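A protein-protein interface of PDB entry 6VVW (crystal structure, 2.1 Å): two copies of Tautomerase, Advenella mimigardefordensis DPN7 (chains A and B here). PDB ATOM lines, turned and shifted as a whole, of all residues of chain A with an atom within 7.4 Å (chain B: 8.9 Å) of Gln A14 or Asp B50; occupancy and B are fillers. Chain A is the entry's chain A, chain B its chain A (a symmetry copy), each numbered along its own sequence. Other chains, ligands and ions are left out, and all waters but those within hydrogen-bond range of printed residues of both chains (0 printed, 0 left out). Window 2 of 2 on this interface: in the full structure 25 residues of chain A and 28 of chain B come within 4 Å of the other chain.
Of the 18 printed residues of chain A, 7 touch a printed residue of chain B.
Hydrophobic or aromatic side chains of chain A that line the printed part of chain B: Leu A21, Leu A43 and His A44.
Of the 19 printed residues of chain B, 7 touch a printed residue of chain A.
Hydrophobic or aromatic side chains of chain B that line the printed part of chain A: His B44, Ile B46 and Ile B52.
Among the printed residues, no Asp or Glu carboxylate lies within 4 Å of a Lys or Arg side-chain nitrogen of the other chain.
Printed residues of chain B within 4 Å of Ile A41: Ser B51 (3.2 Å) and Ile B52 (3.0 Å).
Of the printed residues of chain A, Gln B7 touches Ser A42.
Val B8 touches none of the printed residues of chain A.
Printed residues of chain A within 4 Å of Ile B46: Ser A42.
Of the printed residues of chain A, Asp B50 touches Gln A14 (3.4 Å), Ser A42 (3.7 Å) and Leu A43 (2.8 Å).
His B44 touches its own counterpart, His A44.
Of the 11 pairs that touch across the chains among the printed residues, 1 has its exchanged pair printed and touching as well.
Lys A17 touches Gln B49.
CD1 of Ile B52 touches CB of Leu A21, 3.3 Å away.
Ile A41 touches Ser B51 (O to CA, 3.2 Å).
Ser A42 touches Ile B46.
CA of Ser A42 touches O of Asp B50 (3.7 Å).
His B44 touches His A44 (NE2 to CG, 3.5 Å).
N of Val A6 sits at hydrogen-bond distance from O of Ser A42 (2.9 Å).
The backbone carbonyl oxygen (O) of Gln A14 is in hydrogen-bond range of the side-chain hydroxyl (OG1) of Thr A18 (3.0 Å).
The side-chain amino group of Lys A17 is in salt-bridge range of the side-chain carboxylate of Glu A45.
The backbone NH (N) of Ile B46 sits at hydrogen-bond distance from the backbone carbonyl oxygen (O) of Val B8.
O of Ile B46 lies within hydrogen-bond range of N of Ala B10 (2.5 Å).
The backbone carbonyl oxygen (O) of Ser B51 is in hydrogen-bond range of the backbone NH (N) of Gly B58.
OE1 of Gln A14 sits close to O of Gln B49, 3.2 Å away.
The side-chain carboxylate of Asp B50 is in hydrogen-bond range of the side-chain amide nitrogen of Gln A14, at 3.4 Å.
O of Ile A41 is in hydrogen-bond range of N of Ile B52, at 3.0 Å.
OG of Ser A42 lies within hydrogen-bond range of OE1 of Gln B7 (2.8 Å).
The backbone NH (N) of Leu A43 sits at hydrogen-bond distance from the backbone carbonyl oxygen (O) of Asp B50, 2.8 Å away.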
ATOM      1  N   VAL A   6     -12.504 -13.441   2.642  1.00  0.00           N
ATOM      2  CA  VAL A   6     -13.663 -12.574   2.444  1.00  0.00           C
ATOM      3  C   VAL A   6     -14.558 -12.648   3.667  1.00  0.00           C
ATOM      4  O   VAL A   6     -14.912 -13.745   4.111  1.00  0.00           O
ATOM      5  CB  VAL A   6     -14.478 -12.980   1.202  1.00  0.00           C
ATOM      6  CG1 VAL A   6     -15.440 -11.890   0.849  1.00  0.00           C
ATOM      7  CG2 VAL A   6     -13.579 -13.334   0.037  1.00  0.00           C
ATOM      8  N   ARG A  12     -26.814 -15.976   3.724  1.00  0.00           N
ATOM      9  CA  ARG A  12     -27.007 -16.211   2.304  1.00  0.00           C
ATOM     10  C   ARG A  12     -27.167 -17.700   2.049  1.00  0.00           C
ATOM     11  O   ARG A  12     -26.685 -18.532   2.816  1.00  0.00           O
ATOM     12  CB  ARG A  12     -25.819 -15.685   1.469  1.00  0.00           C
ATOM     13  CG  ARG A  12     -25.269 -14.333   1.863  1.00  0.00           C
ATOM     14  CD  ARG A  12     -26.074 -13.191   1.272  1.00  0.00           C
ATOM     15  NE  ARG A  12     -26.154 -12.079   2.218  1.00  0.00           N
ATOM     16  CZ  ARG A  12     -26.356 -10.808   1.872  1.00  0.00           C
ATOM     17  NH1 ARG A  12     -26.503 -10.477   0.597  1.00  0.00           N
ATOM     18  NH2 ARG A  12     -26.411  -9.863   2.800  1.00  0.00           N
ATOM     19  N   SER A  13     -27.824 -18.028   0.947  1.00  0.00           N
ATOM     20  CA  SER A  13     -27.828 -19.412   0.510  1.00  0.00           C
ATOM     21  C   SER A  13     -26.468 -19.816  -0.023  1.00  0.00           C
ATOM     22  O   SER A  13     -25.666 -18.985  -0.445  1.00  0.00           O
ATOM     23  CB  SER A  13     -28.839 -19.660  -0.593  1.00  0.00           C
ATOM     24  OG  SER A  13     -28.381 -20.761  -1.349  1.00  0.00           O
ATOM     25  N   GLN A  14     -26.236 -21.126  -0.047  1.00  0.00           N
ATOM     26  CA  GLN A  14     -24.969 -21.645  -0.534  1.00  0.00           C
ATOM     27  C   GLN A  14     -24.641 -21.104  -1.909  1.00  0.00           C
ATOM     28  O   GLN A  14     -23.552 -20.587  -2.136  1.00  0.00           O
ATOM     29  CB  GLN A  14     -24.999 -23.167  -0.594  1.00  0.00           C
ATOM     30  CG  GLN A  14     -24.393 -23.841   0.593  1.00  0.00           C
ATOM     31  CD  GLN A  14     -22.987 -23.370   0.883  1.00  0.00           C
ATOM     32  OE1 GLN A  14     -22.345 -22.706   0.055  1.00  0.00           O
ATOM     33  NE2 GLN A  14     -22.492 -23.721   2.064  1.00  0.00           N
ATOM     34  N   GLN A  15     -25.573 -21.231  -2.844  1.00  0.00           N
ATOM     35  CA  GLN A  15     -25.261 -20.923  -4.232  1.00  0.00           C
ATOM     36  C   GLN A  15     -24.868 -19.467  -4.403  1.00  0.00           C
ATOM     37  O   GLN A  15     -24.038 -19.135  -5.255  1.00  0.00           O
ATOM     38  CB  GLN A  15     -26.450 -21.290  -5.113  1.00  0.00           C
ATOM     39  CG  GLN A  15     -26.523 -22.782  -5.324  1.00  0.00           C
ATOM     40  CD  GLN A  15     -25.363 -23.314  -6.142  1.00  0.00           C
ATOM     41  OE1 GLN A  15     -24.818 -22.622  -6.996  1.00  0.00           O
ATOM     42  NE2 GLN A  15     -24.981 -24.552  -5.877  1.00  0.00           N
ATOM     43  N   GLN A  16     -25.442 -18.584  -3.599  1.00  0.00           N
ATOM     44  CA  GLN A  16     -24.894 -17.248  -3.502  1.00  0.00           C
ATOM     45  C   GLN A  16     -23.434 -17.323  -3.096  1.00  0.00           C
ATOM     46  O   GLN A  16     -22.535 -16.980  -3.869  1.00  0.00           O
ATOM     47  CB  GLN A  16     -25.707 -16.438  -2.499  1.00  0.00           C
ATOM     48  CG  GLN A  16     -27.190 -16.381  -2.810  1.00  0.00           C
ATOM     49  CD  GLN A  16     -27.904 -15.440  -1.883  1.00  0.00           C
ATOM     50  OE1 GLN A  16     -27.921 -15.645  -0.673  1.00  0.00           O
ATOM     51  NE2 GLN A  16     -28.487 -14.392  -2.435  1.00  0.00           N
ATOM     52  N   LYS A  17     -23.181 -17.839  -1.905  1.00  0.00           N
ATOM     53  CA  LYS A  17     -21.832 -18.041  -1.411  1.00  0.00           C
ATOM     54  C   LYS A  17     -21.134 -19.211  -2.059  1.00  0.00           C
ATOM     55  O   LYS A  17     -20.080 -19.629  -1.566  1.00  0.00           O
ATOM     56  CB  LYS A  17     -21.869 -18.245   0.093  1.00  0.00           C
ATOM     57  CG  LYS A  17     -22.873 -17.384   0.798  1.00  0.00           C
ATOM     58  CD  LYS A  17     -23.055 -17.888   2.193  1.00  0.00           C
ATOM     59  CE  LYS A  17     -23.520 -19.319   2.164  1.00  0.00           C
ATOM     60  NZ  LYS A  17     -22.797 -20.138   3.159  1.00  0.00           N
ATOM     61  N   THR A  18     -21.710 -19.758  -3.128  1.00  0.00           N
ATOM     62  CA  THR A  18     -21.034 -20.687  -4.018  1.00  0.00           C
ATOM     63  C   THR A  18     -20.685 -20.033  -5.348  1.00  0.00           C
ATOM     64  O   THR A  18     -19.502 -19.881  -5.680  1.00  0.00           O
ATOM     65  CB  THR A  18     -21.901 -21.930  -4.262  1.00  0.00           C
ATOM     66  OG1 THR A  18     -21.784 -22.799  -3.134  1.00  0.00           O
ATOM     67  CG2 THR A  18     -21.457 -22.683  -5.498  1.00  0.00           C
ATOM     68  N   ALA A  19     -21.688 -19.621  -6.119  1.00  0.00           N
ATOM     69  CA  ALA A  19     -21.404 -19.005  -7.404  1.00  0.00           C
ATOM     70  C   ALA A  19     -20.522 -17.779  -7.242  1.00  0.00           C
ATOM     71  O   ALA A  19     -19.682 -17.499  -8.107  1.00  0.00           O
ATOM     72  CB  ALA A  19     -22.703 -18.647  -8.105  1.00  0.00           C
ATOM     73  N   PHE A  20     -20.668 -17.057  -6.129  1.00  0.00           N
ATOM     74  CA  PHE A  20     -19.790 -15.923  -5.884  1.00  0.00           C
ATOM     75  C   PHE A  20     -18.338 -16.356  -5.888  1.00  0.00           C
ATOM     76  O   PHE A  20     -17.482 -15.702  -6.485  1.00  0.00           O
ATOM     77  CB  PHE A  20     -20.134 -15.269  -4.558  1.00  0.00           C
ATOM     78  CG  PHE A  20     -18.952 -14.645  -3.876  1.00  0.00           C
ATOM     79  CD1 PHE A  20     -18.617 -13.331  -4.121  1.00  0.00           C
ATOM     80  CD2 PHE A  20     -18.193 -15.367  -2.975  1.00  0.00           C
ATOM     81  CE1 PHE A  20     -17.555 -12.750  -3.496  1.00  0.00           C
ATOM     82  CE2 PHE A  20     -17.125 -14.799  -2.357  1.00  0.00           C
ATOM     83  CZ  PHE A  20     -16.806 -13.479  -2.620  1.00  0.00           C
ATOM     84  N   LEU A  21     -18.029 -17.451  -5.214  1.00  0.00           N
ATOM     85  CA  LEU A  21     -16.651 -17.889  -5.233  1.00  0.00           C
ATOM     86  C   LEU A  21     -16.280 -18.391  -6.607  1.00  0.00           C
ATOM     87  O   LEU A  21     -15.104 -18.351  -6.990  1.00  0.00           O
ATOM     88  CB  LEU A  21     -16.405 -18.976  -4.192  1.00  0.00           C
ATOM     89  CG  LEU A  21     -16.798 -18.945  -2.713  1.00  0.00           C
ATOM     90  CD1 LEU A  21     -17.055 -20.391  -2.238  1.00  0.00           C
ATOM     91  CD2 LEU A  21     -15.758 -18.266  -1.823  1.00  0.00           C
ATOM     92  N   ILE A  41      -9.825 -18.800  -2.735  1.00  0.00           N
ATOM     93  CA  ILE A  41     -10.750 -17.832  -2.161  1.00  0.00           C
ATOM     94  C   ILE A  41     -11.450 -18.508  -1.010  1.00  0.00           C
ATOM     95  O   ILE A  41     -11.905 -19.646  -1.140  1.00  0.00           O
ATOM     96  CB  ILE A  41     -11.783 -17.335  -3.185  1.00  0.00           C
ATOM     97  CG1 ILE A  41     -11.102 -16.507  -4.266  1.00  0.00           C
ATOM     98  CG2 ILE A  41     -12.829 -16.512  -2.486  1.00  0.00           C
ATOM     99  CD1 ILE A  41     -11.864 -16.424  -5.553  1.00  0.00           C
ATOM    100  N   SER A  42     -11.552 -17.815   0.114  1.00  0.00           N
ATOM    101  CA  SER A  42     -12.196 -18.362   1.298  1.00  0.00           C
ATOM    102  C   SER A  42     -13.277 -17.402   1.761  1.00  0.00           C
ATOM    103  O   SER A  42     -13.001 -16.220   1.972  1.00  0.00           O
ATOM    104  CB  SER A  42     -11.177 -18.573   2.404  1.00  0.00           C
ATOM    105  OG  SER A  42     -11.124 -17.448   3.261  1.00  0.00           O
ATOM    106  N   LEU A  43     -14.494 -17.900   1.957  1.00  0.00           N
ATOM    107  CA  LEU A  43     -15.568 -17.063   2.470  1.00  0.00           C
ATOM    108  C   LEU A  43     -15.878 -17.408   3.921  1.00  0.00           C
ATOM    109  O   LEU A  43     -15.983 -18.589   4.273  1.00  0.00           O
ATOM    110  CB  LEU A  43     -16.832 -17.209   1.618  1.00  0.00           C
ATOM    111  CG  LEU A  43     -17.944 -16.267   2.071  1.00  0.00           C
ATOM    112  CD1 LEU A  43     -17.362 -14.892   2.016  1.00  0.00           C
ATOM    113  CD2 LEU A  43     -19.128 -16.324   1.160  1.00  0.00           C
ATOM    114  N   HIS A  44     -16.058 -16.369   4.753  1.00  0.00           N
ATOM    115  CA  HIS A  44     -16.267 -16.516   6.198  1.00  0.00           C
ATOM    116  C   HIS A  44     -17.356 -15.542   6.632  1.00  0.00           C
ATOM    117  O   HIS A  44     -17.058 -14.391   6.961  1.00  0.00           O
ATOM    118  CB  HIS A  44     -14.965 -16.260   6.937  1.00  0.00           C
ATOM    119  CG  HIS A  44     -15.123 -15.921   8.389  1.00  0.00           C
ATOM    120  ND1 HIS A  44     -16.108 -16.464   9.189  1.00  0.00           N
ATOM    121  CD2 HIS A  44     -14.393 -15.109   9.192  1.00  0.00           C
ATOM    122  CE1 HIS A  44     -15.979 -15.999  10.420  1.00  0.00           C
ATOM    123  NE2 HIS A  44     -14.954 -15.167  10.447  1.00  0.00           N
ATOM    124  N   GLU A  45     -18.606 -16.007   6.659  1.00  0.00           N
ATOM    125  CA  GLU A  45     -19.711 -15.106   6.947  1.00  0.00           C
ATOM    126  C   GLU A  45     -19.685 -14.652   8.396  1.00  0.00           C
ATOM    127  O   GLU A  45     -19.213 -15.350   9.290  1.00  0.00           O
ATOM    128  CB  GLU A  45     -21.061 -15.750   6.671  1.00  0.00           C
ATOM    129  CG  GLU A  45     -21.068 -16.898   5.694  1.00  0.00           C
ATOM    130  CD  GLU A  45     -22.464 -17.472   5.540  1.00  0.00           C
ATOM    131  OE1 GLU A  45     -23.432 -16.716   5.749  1.00  0.00           O
ATOM    132  OE2 GLU A  45     -22.597 -18.661   5.186  1.00  0.00           O
ATOM    133  N   THR A  91     -23.735 -11.567  -7.246  1.00  0.00           N
ATOM    134  CA  THR A  91     -24.021 -12.901  -6.732  1.00  0.00           C
ATOM    135  C   THR A  91     -23.997 -13.005  -5.210  1.00  0.00           C
ATOM    136  O   THR A  91     -24.368 -14.055  -4.676  1.00  0.00           O
ATOM    137  CB  THR A  91     -23.037 -13.899  -7.364  1.00  0.00           C
ATOM    138  OG1 THR A  91     -23.067 -13.719  -8.777  1.00  0.00           O
ATOM    139  CG2 THR A  91     -23.423 -15.320  -7.104  1.00  0.00           C
ATOM    140  N   LEU A  92     -23.607 -11.953  -4.487  1.00  0.00           N
ATOM    141  CA  LEU A  92     -23.835 -11.906  -3.050  1.00  0.00           C
ATOM    142  C   LEU A  92     -25.037 -11.063  -2.667  1.00  0.00           C
ATOM    143  O   LEU A  92     -25.397 -11.036  -1.488  1.00  0.00           O
ATOM    144  CB  LEU A  92     -22.612 -11.357  -2.316  1.00  0.00           C
ATOM    145  CG  LEU A  92     -21.338 -12.186  -2.264  1.00  0.00           C
ATOM    146  CD1 LEU A  92     -20.340 -11.477  -1.379  1.00  0.00           C
ATOM    147  CD2 LEU A  92     -21.602 -13.596  -1.743  1.00  0.00           C
ATOM    148  N   GLN B   7      -6.074 -20.546   8.115  1.00  0.00           N
ATOM    149  CA  GLN B   7      -7.278 -21.160   7.578  1.00  0.00           C
ATOM    150  C   GLN B   7      -6.926 -22.543   7.058  1.00  0.00           C
ATOM    151  O   GLN B   7      -6.059 -22.679   6.191  1.00  0.00           O
ATOM    152  CB  GLN B   7      -7.884 -20.314   6.467  1.00  0.00           C
ATOM    153  CG  GLN B   7      -8.575 -19.080   6.980  1.00  0.00           C
ATOM    154  CD  GLN B   7      -9.045 -18.136   5.877  1.00  0.00           C
ATOM    155  OE1 GLN B   7      -8.918 -18.425   4.682  1.00  0.00           O
ATOM    156  NE2 GLN B   7      -9.603 -16.987   6.284  1.00  0.00           N
ATOM    157  N   VAL B   8      -7.585 -23.566   7.600  1.00  0.00           N
ATOM    158  CA  VAL B   8      -7.448 -24.927   7.101  1.00  0.00           C
ATOM    159  C   VAL B   8      -8.799 -25.385   6.584  1.00  0.00           C
ATOM    160  O   VAL B   8      -9.834 -24.969   7.099  1.00  0.00           O
ATOM    161  CB  VAL B   8      -6.944 -25.875   8.201  1.00  0.00           C
ATOM    162  CG1 VAL B   8      -7.837 -25.777   9.401  1.00  0.00           C
ATOM    163  CG2 VAL B   8      -6.891 -27.302   7.682  1.00  0.00           C
ATOM    164  N   THR B   9      -8.801 -26.234   5.565  1.00  0.00           N
ATOM    165  CA  THR B   9     -10.057 -26.861   5.167  1.00  0.00           C
ATOM    166  C   THR B   9     -10.646 -27.590   6.379  1.00  0.00           C
ATOM    167  O   THR B   9      -9.918 -28.180   7.182  1.00  0.00           O
ATOM    168  CB  THR B   9      -9.833 -27.821   3.988  1.00  0.00           C
ATOM    169  OG1 THR B   9     -11.039 -27.966   3.234  1.00  0.00           O
ATOM    170  CG2 THR B   9      -9.437 -29.198   4.452  1.00  0.00           C
ATOM    171  N   ALA B  10     -11.963 -27.495   6.561  1.00  0.00           N
ATOM    172  CA  ALA B  10     -12.552 -28.043   7.774  1.00  0.00           C
ATOM    173  C   ALA B  10     -12.452 -29.565   7.795  1.00  0.00           C
ATOM    174  O   ALA B  10     -12.339 -30.221   6.751  1.00  0.00           O
ATOM    175  CB  ALA B  10     -14.016 -27.626   7.894  1.00  0.00           C
ATOM    176  N   HIS B  44      -8.662 -21.413  12.341  1.00  0.00           N
ATOM    177  CA  HIS B  44     -10.048 -21.106  11.972  1.00  0.00           C
ATOM    178  C   HIS B  44     -10.433 -21.967  10.775  1.00  0.00           C
ATOM    179  O   HIS B  44     -10.215 -21.564   9.630  1.00  0.00           O
ATOM    180  CB  HIS B  44     -10.184 -19.626  11.658  1.00  0.00           C
ATOM    181  CG  HIS B  44     -11.386 -19.264  10.840  1.00  0.00           C
ATOM    182  ND1 HIS B  44     -12.600 -19.912  10.953  1.00  0.00           N
ATOM    183  CD2 HIS B  44     -11.566 -18.293   9.910  1.00  0.00           C
ATOM    184  CE1 HIS B  44     -13.472 -19.359  10.127  1.00  0.00           C
ATOM    185  NE2 HIS B  44     -12.867 -18.382   9.476  1.00  0.00           N
ATOM    186  N   GLU B  45     -11.027 -23.132  11.036  1.00  0.00           N
ATOM    187  CA  GLU B  45     -11.315 -24.060   9.953  1.00  0.00           C
ATOM    188  C   GLU B  45     -12.416 -23.527   9.052  1.00  0.00           C
ATOM    189  O   GLU B  45     -13.295 -22.779   9.470  1.00  0.00           O
ATOM    190  CB  GLU B  45     -11.740 -25.427  10.469  1.00  0.00           C
ATOM    191  CG  GLU B  45     -11.295 -25.784  11.863  1.00  0.00           C
ATOM    192  CD  GLU B  45     -11.815 -27.150  12.268  1.00  0.00           C
ATOM    193  OE1 GLU B  45     -12.042 -27.978  11.365  1.00  0.00           O
ATOM    194  OE2 GLU B  45     -11.972 -27.408  13.479  1.00  0.00           O
ATOM    195  N   ILE B  46     -12.376 -23.963   7.803  1.00  0.00           N
ATOM    196  CA  ILE B  46     -13.188 -23.407   6.737  1.00  0.00           C
ATOM    197  C   ILE B  46     -13.932 -24.552   6.075  1.00  0.00           C
ATOM    198  O   ILE B  46     -13.336 -25.586   5.758  1.00  0.00           O
ATOM    199  CB  ILE B  46     -12.328 -22.658   5.704  1.00  0.00           C
ATOM    200  CG1 ILE B  46     -11.666 -21.439   6.340  1.00  0.00           C
ATOM    201  CG2 ILE B  46     -13.175 -22.226   4.550  1.00  0.00           C
ATOM    202  CD1 ILE B  46     -11.370 -20.365   5.353  1.00  0.00           C
ATOM    203  N   GLU B  47     -15.228 -24.374   5.880  1.00  0.00           N
ATOM    204  CA  GLU B  47     -16.021 -25.423   5.274  1.00  0.00           C
ATOM    205  C   GLU B  47     -15.696 -25.534   3.799  1.00  0.00           C
ATOM    206  O   GLU B  47     -15.474 -24.530   3.117  1.00  0.00           O
ATOM    207  CB  GLU B  47     -17.516 -25.139   5.436  1.00  0.00           C
ATOM    208  CG  GLU B  47     -18.206 -25.948   6.497  1.00  0.00           C
ATOM    209  CD  GLU B  47     -18.030 -27.440   6.299  1.00  0.00           C
ATOM    210  OE1 GLU B  47     -17.901 -27.889   5.139  1.00  0.00           O
ATOM    211  OE2 GLU B  47     -18.028 -28.161   7.314  1.00  0.00           O
ATOM    212  N   GLN B  48     -15.703 -26.771   3.297  1.00  0.00           N
ATOM    213  CA  GLN B  48     -15.863 -26.971   1.868  1.00  0.00           C
ATOM    214  C   GLN B  48     -17.101 -26.188   1.455  1.00  0.00           C
ATOM    215  O   GLN B  48     -17.873 -25.746   2.312  1.00  0.00           O
ATOM    216  CB  GLN B  48     -15.973 -28.456   1.531  1.00  0.00           C
ATOM    217  CG  GLN B  48     -15.081 -29.339   2.397  1.00  0.00           C
ATOM    218  CD  GLN B  48     -14.520 -30.553   1.670  1.00  0.00           C
ATOM    219  OE1 GLN B  48     -15.184 -31.151   0.827  1.00  0.00           O
ATOM    220  NE2 GLN B  48     -13.275 -30.921   1.996  1.00  0.00           N
ATOM    221  N   GLN B  49     -17.267 -25.947   0.165  1.00  0.00           N
ATOM    222  CA  GLN B  49     -18.229 -24.979  -0.361  1.00  0.00           C
ATOM    223  C   GLN B  49     -18.261 -23.661   0.413  1.00  0.00           C
ATOM    224  O   GLN B  49     -19.187 -22.860   0.254  1.00  0.00           O
ATOM    225  CB  GLN B  49     -19.627 -25.611  -0.458  1.00  0.00           C
ATOM    226  CG  GLN B  49     -20.358 -25.892   0.830  1.00  0.00           C
ATOM    227  CD  GLN B  49     -21.069 -27.227   0.770  1.00  0.00           C
ATOM    228  OE1 GLN B  49     -22.191 -27.318   0.279  1.00  0.00           O
ATOM    229  NE2 GLN B  49     -20.403 -28.279   1.250  1.00  0.00           N
ATOM    230  N   ASP B  50     -17.249 -23.419   1.245  1.00  0.00           N
ATOM    231  CA  ASP B  50     -16.919 -22.083   1.721  1.00  0.00           C
ATOM    232  C   ASP B  50     -15.488 -21.708   1.349  1.00  0.00           C
ATOM    233  O   ASP B  50     -14.970 -20.706   1.862  1.00  0.00           O
ATOM    234  CB  ASP B  50     -17.108 -21.966   3.240  1.00  0.00           C
ATOM    235  CG  ASP B  50     -18.560 -22.064   3.665  1.00  0.00           C
ATOM    236  OD1 ASP B  50     -19.357 -22.715   2.962  1.00  0.00           O
ATOM    237  OD2 ASP B  50     -18.911 -21.487   4.709  1.00  0.00           O
ATOM    238  N   SER B  51     -14.834 -22.502   0.492  1.00  0.00           N
ATOM    239  CA  SER B  51     -13.503 -22.204  -0.029  1.00  0.00           C
ATOM    240  C   SER B  51     -13.322 -22.849  -1.397  1.00  0.00           C
ATOM    241  O   SER B  51     -14.088 -23.726  -1.785  1.00  0.00           O
ATOM    242  CB  SER B  51     -12.409 -22.698   0.905  1.00  0.00           C
ATOM    243  OG  SER B  51     -12.192 -24.077   0.680  1.00  0.00           O
ATOM    244  N   ILE B  52     -12.283 -22.401  -2.127  1.00  0.00           N
ATOM    245  CA  ILE B  52     -11.918 -22.890  -3.461  1.00  0.00           C
ATOM    246  C   ILE B  52     -10.415 -22.813  -3.685  1.00  0.00           C
ATOM    247  O   ILE B  52      -9.848 -21.722  -3.648  1.00  0.00           O
ATOM    248  CB  ILE B  52     -12.567 -22.080  -4.593  1.00  0.00           C
ATOM    249  CG1 ILE B  52     -14.036 -21.795  -4.372  1.00  0.00           C
ATOM    250  CG2 ILE B  52     -12.366 -22.779  -5.913  1.00  0.00           C
ATOM    251  CD1 ILE B  52     -14.709 -21.409  -5.655  1.00  0.00           C
ATOM    252  N   VAL B  53      -9.768 -23.931  -4.011  1.00  0.00           N
ATOM    253  CA  VAL B  53      -8.374 -23.945  -4.447  1.00  0.00           C
ATOM    254  C   VAL B  53      -8.350 -24.311  -5.919  1.00  0.00           C
ATOM    255  O   VAL B  53      -9.082 -25.208  -6.349  1.00  0.00           O
ATOM    256  CB  VAL B  53      -7.511 -24.918  -3.626  1.00  0.00           C
ATOM    257  CG1 VAL B  53      -6.321 -25.436  -4.444  1.00  0.00           C
ATOM    258  CG2 VAL B  53      -7.024 -24.231  -2.374  1.00  0.00           C
ATOM    259  N   GLN B  56     -11.764 -25.324  -8.041  1.00  0.00           N
ATOM    260  CA  GLN B  56     -12.621 -26.413  -7.607  1.00  0.00           C
ATOM    261  C   GLN B  56     -13.036 -26.152  -6.173  1.00  0.00           C
ATOM    262  O   GLN B  56     -12.217 -26.247  -5.264  1.00  0.00           O
ATOM    263  CB  GLN B  56     -11.922 -27.755  -7.772  1.00  0.00           C
ATOM    264  CG  GLN B  56     -10.458 -27.708  -7.566  1.00  0.00           C
ATOM    265  CD  GLN B  56      -9.925 -29.063  -7.224  1.00  0.00           C
ATOM    266  OE1 GLN B  56     -10.679 -30.035  -7.202  1.00  0.00           O
ATOM    267  NE2 GLN B  56      -8.635 -29.143  -6.906  1.00  0.00           N
ATOM    268  N   VAL B  57     -14.304 -25.800  -5.976  1.00  0.00           N
ATOM    269  CA  VAL B  57     -14.789 -25.591  -4.629  1.00  0.00           C
ATOM    270  C   VAL B  57     -14.587 -26.885  -3.870  1.00  0.00           C
ATOM    271  O   VAL B  57     -14.520 -27.973  -4.459  1.00  0.00           O
ATOM    272  CB  VAL B  57     -16.266 -25.173  -4.606  1.00  0.00           C
ATOM    273  CG1 VAL B  57     -16.609 -24.500  -3.303  1.00  0.00           C
ATOM    274  CG2 VAL B  57     -16.567 -24.283  -5.756  1.00  0.00           C
ATOM    275  N   GLY B  58     -14.472 -26.776  -2.557  1.00  0.00           N
ATOM    276  CA  GLY B  58     -14.016 -27.916  -1.799  1.00  0.00           C
ATOM    277  C   GLY B  58     -12.720 -28.442  -2.368  1.00  0.00           C
ATOM    278  O   GLY B  58     -12.716 -29.273  -3.286  1.00  0.00           O
ATOM    279  N   ALA B  59     -11.615 -27.917  -1.848  1.00  0.00           N
ATOM    280  CA  ALA B  59     -10.283 -28.468  -2.083  1.00  0.00           C
ATOM    281  C   ALA B  59      -9.455 -28.184  -0.841  1.00  0.00           C
ATOM    282  O   ALA B  59      -9.369 -27.029  -0.420  1.00  0.00           O
ATOM    283  CB  ALA B  59      -9.642 -27.857  -3.328  1.00  0.00           C
ATOM    284  N   PHE B  61      -7.055 -27.179   2.029  1.00  0.00           N
ATOM    285  CA  PHE B  61      -6.200 -26.016   1.916  1.00  0.00           C
ATOM    286  C   PHE B  61      -5.800 -25.530   3.289  1.00  0.00           C
ATOM    287  O   PHE B  61      -6.493 -25.752   4.281  1.00  0.00           O
ATOM    288  CB  PHE B  61      -6.896 -24.885   1.182  1.00  0.00           C
ATOM    289  CG  PHE B  61      -7.654 -24.002   2.084  1.00  0.00           C
ATOM    290  CD1 PHE B  61      -8.893 -24.384   2.546  1.00  0.00           C
ATOM    291  CD2 PHE B  61      -7.127 -22.795   2.495  1.00  0.00           C
ATOM    292  CE1 PHE B  61      -9.606 -23.578   3.396  1.00  0.00           C
ATOM    293  CE2 PHE B  61      -7.828 -21.990   3.347  1.00  0.00           C
ATOM    294  CZ  PHE B  61      -9.083 -22.378   3.795  1.00  0.00           C
